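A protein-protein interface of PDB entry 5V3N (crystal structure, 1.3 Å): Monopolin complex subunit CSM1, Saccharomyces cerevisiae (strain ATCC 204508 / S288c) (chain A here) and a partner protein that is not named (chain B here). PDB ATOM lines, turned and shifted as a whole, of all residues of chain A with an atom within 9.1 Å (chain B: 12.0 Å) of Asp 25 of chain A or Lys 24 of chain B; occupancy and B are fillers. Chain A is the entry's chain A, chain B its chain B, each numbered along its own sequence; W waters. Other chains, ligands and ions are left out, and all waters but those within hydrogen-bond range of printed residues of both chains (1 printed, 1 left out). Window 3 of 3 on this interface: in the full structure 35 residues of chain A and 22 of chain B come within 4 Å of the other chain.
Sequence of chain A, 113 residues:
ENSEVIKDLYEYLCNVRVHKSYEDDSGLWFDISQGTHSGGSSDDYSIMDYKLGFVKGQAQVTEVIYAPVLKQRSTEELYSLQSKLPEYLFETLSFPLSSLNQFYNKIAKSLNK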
ATOM      1  N   TYR A  22      -1.045  23.590  13.545  1.00  0.00           N
ATOM      2  CA  TYR A  22       0.193  24.080  14.156  1.00  0.00           C
ATOM      3  C   TYR A  22       0.293  23.625  15.589  1.00  0.00           C
ATOM      4  O   TYR A  22      -0.729  23.260  16.175  1.00  0.00           O
ATOM      5  CB  TYR A  22       0.241  25.629  14.080  1.00  0.00           C
ATOM      6  CG  TYR A  22      -0.909  26.288  14.868  1.00  0.00           C
ATOM      7  CD1 TYR A  22      -0.728  26.729  16.149  1.00  0.00           C
ATOM      8  CD2 TYR A  22      -2.090  26.539  14.230  1.00  0.00           C
ATOM      9  CE1 TYR A  22      -1.785  27.309  16.860  1.00  0.00           C
ATOM     10  CE2 TYR A  22      -3.172  27.118  14.915  1.00  0.00           C
ATOM     11  CZ  TYR A  22      -2.978  27.482  16.223  1.00  0.00           C
ATOM     12  OH  TYR A  22      -4.086  28.067  16.820  1.00  0.00           O
ATOM     13  N   GLU A  23       1.484  23.546  16.149  1.00  0.00           N
ATOM     14  CA  GLU A  23       1.714  23.166  17.492  1.00  0.00           C
ATOM     15  C   GLU A  23       2.247  24.371  18.249  1.00  0.00           C
ATOM     16  O   GLU A  23       3.246  24.951  17.798  1.00  0.00           O
ATOM     17  CB  GLU A  23       2.595  21.925  17.605  1.00  0.00           C
ATOM     18  CG  GLU A  23       2.778  21.430  18.942  1.00  0.00           C
ATOM     19  CD  GLU A  23       3.597  20.170  19.121  1.00  0.00           C
ATOM     20  OE1 GLU A  23       4.190  19.616  18.136  1.00  0.00           O
ATOM     21  OE2 GLU A  23       3.676  19.752  20.322  1.00  0.00           O
ATOM     22  N   ASP A  24       1.670  24.791  19.361  1.00  0.00           N
ATOM     23  CA  ASP A  24       2.054  25.991  20.098  1.00  0.00           C
ATOM     24  C   ASP A  24       2.342  25.554  21.536  1.00  0.00           C
ATOM     25  O   ASP A  24       2.593  24.352  21.809  1.00  0.00           O
ATOM     26  CB  ASP A  24       1.031  27.167  19.936  1.00  0.00           C
ATOM     27  CG  ASP A  24      -0.295  26.967  20.631  1.00  0.00           C
ATOM     28  OD1 ASP A  24      -0.479  25.959  21.342  1.00  0.00           O
ATOM     29  OD2 ASP A  24      -1.179  27.878  20.459  1.00  0.00           O
ATOM     30  N   ASP A  25       2.314  26.536  22.437  1.00  0.00           N
ATOM     31  CA  ASP A  25       2.673  26.344  23.849  1.00  0.00           C
ATOM     32  C   ASP A  25       1.613  25.531  24.570  1.00  0.00           C
ATOM     33  O   ASP A  25       1.905  24.989  25.631  1.00  0.00           O
ATOM     34  CB  ASP A  25       2.857  27.693  24.551  1.00  0.00           C
ATOM     35  CG  ASP A  25       1.633  28.613  24.419  1.00  0.00           C
ATOM     36  OD1 ASP A  25       1.262  28.916  23.261  1.00  0.00           O
ATOM     37  OD2 ASP A  25       1.039  29.015  25.469  1.00  0.00           O
ATOM     38  N   SER A  26       0.394  25.491  24.075  1.00  0.00           N
ATOM     39  CA  SER A  26      -0.632  24.692  24.757  1.00  0.00           C
ATOM     40  C   SER A  26      -0.869  23.284  24.140  1.00  0.00           C
ATOM     41  O   SER A  26      -1.344  22.380  24.839  1.00  0.00           O
ATOM     42  CB  SER A  26      -1.901  25.542  24.940  1.00  0.00           C
ATOM     43  OG  SER A  26      -2.553  25.754  23.692  1.00  0.00           O
ATOM     44  N   GLY A  27      -0.570  23.045  22.885  1.00  0.00           N
ATOM     45  CA  GLY A  27      -0.826  21.751  22.266  1.00  0.00           C
ATOM     46  C   GLY A  27      -0.903  21.831  20.757  1.00  0.00           C
ATOM     47  O   GLY A  27      -0.278  22.692  20.152  1.00  0.00           O
ATOM     48  N   LEU A  28      -1.647  20.900  20.158  1.00  0.00           N
ATOM     49  CA  LEU A  28      -1.746  20.731  18.723  1.00  0.00           C
ATOM     50  C   LEU A  28      -3.073  21.348  18.268  1.00  0.00           C
ATOM     51  O   LEU A  28      -4.138  20.924  18.791  1.00  0.00           O
ATOM     52  CB  LEU A  28      -1.685  19.275  18.304  1.00  0.00           C
ATOM     53  CG  LEU A  28      -1.941  18.960  16.850  1.00  0.00           C
ATOM     54  CD1 LEU A  28      -0.815  19.583  15.994  1.00  0.00           C
ATOM     55  CD2 LEU A  28      -2.002  17.456  16.660  1.00  0.00           C
ATOM     56  N   TRP A  29      -3.081  22.261  17.352  1.00  0.00           N
ATOM     57  CA  TRP A  29      -4.259  23.052  16.981  1.00  0.00           C
ATOM     58  C   TRP A  29      -4.571  22.950  15.531  1.00  0.00           C
ATOM     59  O   TRP A  29      -3.658  22.862  14.695  1.00  0.00           O
ATOM     60  CB  TRP A  29      -4.064  24.510  17.397  1.00  0.00           C
ATOM     61  CG  TRP A  29      -4.048  24.727  18.855  1.00  0.00           C
ATOM     62  CD1 TRP A  29      -2.973  24.695  19.700  1.00  0.00           C
ATOM     63  CD2 TRP A  29      -5.194  24.963  19.673  1.00  0.00           C
ATOM     64  NE1 TRP A  29      -3.362  24.907  21.010  1.00  0.00           N
ATOM     65  CE2 TRP A  29      -4.726  25.120  21.011  1.00  0.00           C
ATOM     66  CE3 TRP A  29      -6.572  25.141  19.405  1.00  0.00           C
ATOM     67  CZ2 TRP A  29      -5.614  25.297  22.077  1.00  0.00           C
ATOM     68  CZ3 TRP A  29      -7.424  25.334  20.477  1.00  0.00           C
ATOM     69  CH2 TRP A  29      -6.928  25.462  21.760  1.00  0.00           C
ATOM     70  N   LYS A  51     -11.572  26.731  16.157  1.00  0.00           N
ATOM     71  CA  LYS A  51     -10.283  26.111  16.442  1.00  0.00           C
ATOM     72  C   LYS A  51     -10.529  24.884  17.276  1.00  0.00           C
ATOM     73  O   LYS A  51     -11.436  24.875  18.142  1.00  0.00           O
ATOM     74  CB  LYS A  51      -9.403  27.032  17.246  1.00  0.00           C
ATOM     75  CG  LYS A  51      -8.898  28.187  16.340  1.00  0.00           C
ATOM     76  CD  LYS A  51      -7.862  28.977  17.087  1.00  0.00           C
ATOM     77  CE  LYS A  51      -7.139  30.042  16.290  1.00  0.00           C
ATOM     78  NZ  LYS A  51      -6.117  29.551  15.373  1.00  0.00           N
ATOM     79  N   PHE A  54      -5.782  20.002  20.826  1.00  0.00           N
ATOM     80  CA  PHE A  54      -5.521  18.769  21.493  1.00  0.00           C
ATOM     81  C   PHE A  54      -4.452  19.076  22.536  1.00  0.00           C
ATOM     82  O   PHE A  54      -3.307  19.429  22.172  1.00  0.00           O
ATOM     83  CB  PHE A  54      -5.139  17.668  20.511  1.00  0.00           C
ATOM     84  CG  PHE A  54      -6.236  17.391  19.541  1.00  0.00           C
ATOM     85  CD1 PHE A  54      -6.454  18.162  18.455  1.00  0.00           C
ATOM     86  CD2 PHE A  54      -7.145  16.422  19.849  1.00  0.00           C
ATOM     87  CE1 PHE A  54      -7.542  17.957  17.649  1.00  0.00           C
ATOM     88  CE2 PHE A  54      -8.227  16.197  19.024  1.00  0.00           C
ATOM     89  CZ  PHE A  54      -8.398  16.934  17.916  1.00  0.00           C
ATOM     90  N   VAL A  55      -4.790  18.939  23.794  1.00  0.00           N
ATOM     91  CA  VAL A  55      -3.976  19.443  24.868  1.00  0.00           C
ATOM     92  C   VAL A  55      -3.784  18.357  25.868  1.00  0.00           C
ATOM     93  O   VAL A  55      -4.683  17.570  26.134  1.00  0.00           O
ATOM     94  CB  VAL A  55      -4.498  20.741  25.554  1.00  0.00           C
ATOM     95  CG1 VAL A  55      -4.799  21.846  24.504  1.00  0.00           C
ATOM     96  CG2 VAL A  55      -5.814  20.514  26.244  1.00  0.00           C
ATOM     97  N   LYS A  56      -2.622  18.342  26.503  1.00  0.00           N
ATOM     98  CA  LYS A  56      -2.445  17.409  27.604  1.00  0.00           C
ATOM     99  C   LYS A  56      -3.099  18.010  28.823  1.00  0.00           C
ATOM    100  O   LYS A  56      -2.668  19.063  29.303  1.00  0.00           O
ATOM    101  CB  LYS A  56      -0.959  17.143  27.807  1.00  0.00           C
ATOM    102  CG  LYS A  56      -0.338  16.660  26.528  1.00  0.00           C
ATOM    103  CD  LYS A  56      -1.133  15.504  25.827  1.00  0.00           C
ATOM    104  CE  LYS A  56      -0.437  14.183  26.049  1.00  0.00           C
ATOM    105  NZ  LYS A  56      -1.252  13.029  25.538  1.00  0.00           N
ATOM    106  N   ALA A  67     -12.955  26.018  20.286  1.00  0.00           N
ATOM    107  CA  ALA A  67     -13.078  27.454  20.476  1.00  0.00           C
ATOM    108  C   ALA A  67     -13.744  28.031  19.240  1.00  0.00           C
ATOM    109  O   ALA A  67     -13.108  28.096  18.167  1.00  0.00           O
ATOM    110  CB  ALA A  67     -11.649  28.014  20.614  1.00  0.00           C
ATOM    111  N   PHE B  18      -9.984  33.260  10.233  1.00  0.00           N
ATOM    112  CA  PHE B  18      -9.087  33.052  11.365  1.00  0.00           C
ATOM    113  C   PHE B  18      -8.087  34.172  11.529  1.00  0.00           C
ATOM    114  O   PHE B  18      -7.324  34.180  12.503  1.00  0.00           O
ATOM    115  CB  PHE B  18      -8.406  31.680  11.217  1.00  0.00           C
ATOM    116  CG  PHE B  18      -9.407  30.528  11.368  1.00  0.00           C
ATOM    117  CD1 PHE B  18     -10.084  30.099  10.282  1.00  0.00           C
ATOM    118  CD2 PHE B  18      -9.605  29.919  12.578  1.00  0.00           C
ATOM    119  CE1 PHE B  18     -11.067  29.108  10.367  1.00  0.00           C
ATOM    120  CE2 PHE B  18     -10.556  28.903  12.665  1.00  0.00           C
ATOM    121  CZ  PHE B  18     -11.285  28.490  11.570  1.00  0.00           C
ATOM    122  N   GLY B  20      -6.166  37.065  12.786  1.00  0.00           N
ATOM    123  CA  GLY B  20      -6.168  37.862  14.001  1.00  0.00           C
ATOM    124  C   GLY B  20      -6.642  37.152  15.251  1.00  0.00           C
ATOM    125  O   GLY B  20      -6.660  37.774  16.322  1.00  0.00           O
ATOM    126  N   VAL B  21      -7.013  35.878  15.157  1.00  0.00           N
ATOM    127  CA  VAL B  21      -7.472  35.100  16.302  1.00  0.00           C
ATOM    128  C   VAL B  21      -6.295  34.337  16.911  1.00  0.00           C
ATOM    129  O   VAL B  21      -5.619  33.574  16.211  1.00  0.00           O
ATOM    130  CB  VAL B  21      -8.561  34.114  15.858  1.00  0.00           C
ATOM    131  CG1 VAL B  21      -9.060  33.305  17.053  1.00  0.00           C
ATOM    132  CG2 VAL B  21      -9.740  34.851  15.085  1.00  0.00           C
ATOM    133  N   SER B  22      -6.108  34.454  18.232  1.00  0.00           N
ATOM    134  CA  SER B  22      -5.082  33.685  18.940  1.00  0.00           C
ATOM    135  C   SER B  22      -5.684  32.510  19.718  1.00  0.00           C
ATOM    136  O   SER B  22      -6.800  32.605  20.233  1.00  0.00           O
ATOM    137  CB  SER B  22      -4.366  34.569  19.945  1.00  0.00           C
ATOM    138  OG  SER B  22      -3.683  33.753  20.883  1.00  0.00           O
ATOM    139  N   SER B  23      -4.926  31.393  19.819  1.00  0.00           N
ATOM    140  CA  SER B  23      -5.297  30.282  20.712  1.00  0.00           C
ATOM    141  C   SER B  23      -4.656  30.380  22.090  1.00  0.00           C
ATOM    142  O   SER B  23      -4.846  29.479  22.914  1.00  0.00           O
ATOM    143  CB  SER B  23      -5.033  28.877  20.100  1.00  0.00           C
ATOM    144  OG  SER B  23      -3.713  28.661  19.579  1.00  0.00           O
ATOM    145  N   LYS B  24      -3.918  31.447  22.371  1.00  0.00           N
ATOM    146  CA  LYS B  24      -3.311  31.609  23.699  1.00  0.00           C
ATOM    147  C   LYS B  24      -4.327  32.085  24.728  1.00  0.00           C
ATOM    148  O   LYS B  24      -5.007  33.083  24.499  1.00  0.00           O
ATOM    149  CB  LYS B  24      -2.160  32.605  23.620  1.00  0.00           C
ATOM    150  CG  LYS B  24      -1.017  32.116  22.760  1.00  0.00           C
ATOM    151  CD  LYS B  24       0.079  33.163  22.701  1.00  0.00           C
ATOM    152  CE  LYS B  24       1.199  32.719  21.769  1.00  0.00           C
ATOM    153  NZ  LYS B  24       1.615  31.314  22.023  1.00  0.00           N
ATOM    154  N   ASN B  29     -10.573  28.719  30.474  1.00  0.00           N
ATOM    155  CA  ASN B  29     -11.963  28.730  30.909  1.00  0.00           C
ATOM    156  C   ASN B  29     -12.845  28.008  29.905  1.00  0.00           C
ATOM    157  O   ASN B  29     -13.325  28.631  28.964  1.00  0.00           O
ATOM    158  CB  ASN B  29     -12.450  30.162  31.071  1.00  0.00           C
ATOM    159  N   CYS B  30     -13.061  26.700  30.111  1.00  0.00           N
ATOM    160  CA  CYS B  30     -13.792  25.869  29.174  1.00  0.00           C
ATOM    161  C   CYS B  30     -14.961  25.226  29.935  1.00  0.00           C
ATOM    162  O   CYS B  30     -14.848  24.904  31.119  1.00  0.00           O
ATOM    163  CB  CYS B  30     -12.931  24.721  28.563  1.00  0.00           C
ATOM    164  SG  CYS B  30     -11.415  25.134  27.832  1.00  0.00           S
HETATM  165  O   HOH W   1      -5.506  32.063  14.004  1.00  0.00           O
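The side-chain hydroxyl of Tyr 22 of chain A sits at hydrogen-bond distance from the side-chain hydroxyl of Ser 23 of chain B, 2.8 Å away. The side-chain carboxylate (OD2) of Asp 24 of chain A is in hydrogen-bond range of the side-chain hydroxyl (OG) of Ser 23 of chain B, at 2.8 Å. The side-chain carboxylate (OD1) of Asp 25 of chain A is in salt-bridge range of the side-chain amino group (NZ) of Lys 24 of chain B (2.7 Å).
The backbone NH (N) of Trp 29 of chain A lies within hydrogen-bond range of the backbone carbonyl oxygen (O) of Tyr 22 of chain A (2.8 Å). The side-chain hydroxyl (OH) of Tyr 22 of chain A is in hydrogen-bond range of the side-chain amino group (NZ) of Lys 51 of chain A (2.9 Å). The side-chain carboxylate of Asp 24 of chain A is in hydrogen-bond range of the backbone NH of Ser 26 of chain A (2.9 Å). The side-chain carboxylate (OD1) of Asp 24 of chain A is in hydrogen-bond range of the indole nitrogen (NE1) of Trp 29 of chain A (3.1 Å). OG of Ser 26 of chain A sits at hydrogen-bond distance from NE1 of Trp 29 of chain A (2.9 Å). N of Ala 67 of chain A is in hydrogen-bond range of O of Lys 51 of chain A, at 2.9 Å.
Trp 29 of chain A touches Ser 23 of chain B (CE2 to CB, 3.9 Å). CE of Lys 51 of chain A touches O of Val 21 of chain B, at 3.8 Å.
Asp 24 of chain A touches just one residue of chain B: Ser 23 (2.8 Å). Of chain B, only Lys 24 comes within 4 Å of Asp 25 of chain A. Printed residues of chain B within 4 Å of Trp 29 of chain A: Ser 23 (3.9 Å). Printed residues of chain B within 4 Å of Lys 51 of chain A: Val 21. Lys 24 of chain B touches just one residue of chain A: Asp 25 (2.7 Å).
Hydrophobic or aromatic side chains of chain B within 4 Å of the printed part of chain A: Val 21. Along chain B the printed residues that touch a printed residue of chain A span positions 21 to 24. Of the 13 printed residues of chain A, 5 touch a printed residue of chain B. Hydrophobic or aromatic side chains of chain A that line the printed part of chain B: Tyr 22 and Trp 29. Among the printed residues, Asp or Glu carboxylates within 4 Å of a Lys or Arg side-chain nitrogen of the other chain: Asp 25 of chain A with Lys 24 of chain B (2.7 Å).
Water W1 lies within hydrogen-bond range of O of Val 21 of chain B, NZ of Lys 51 of chain A and O of Phe 18 of chain B.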
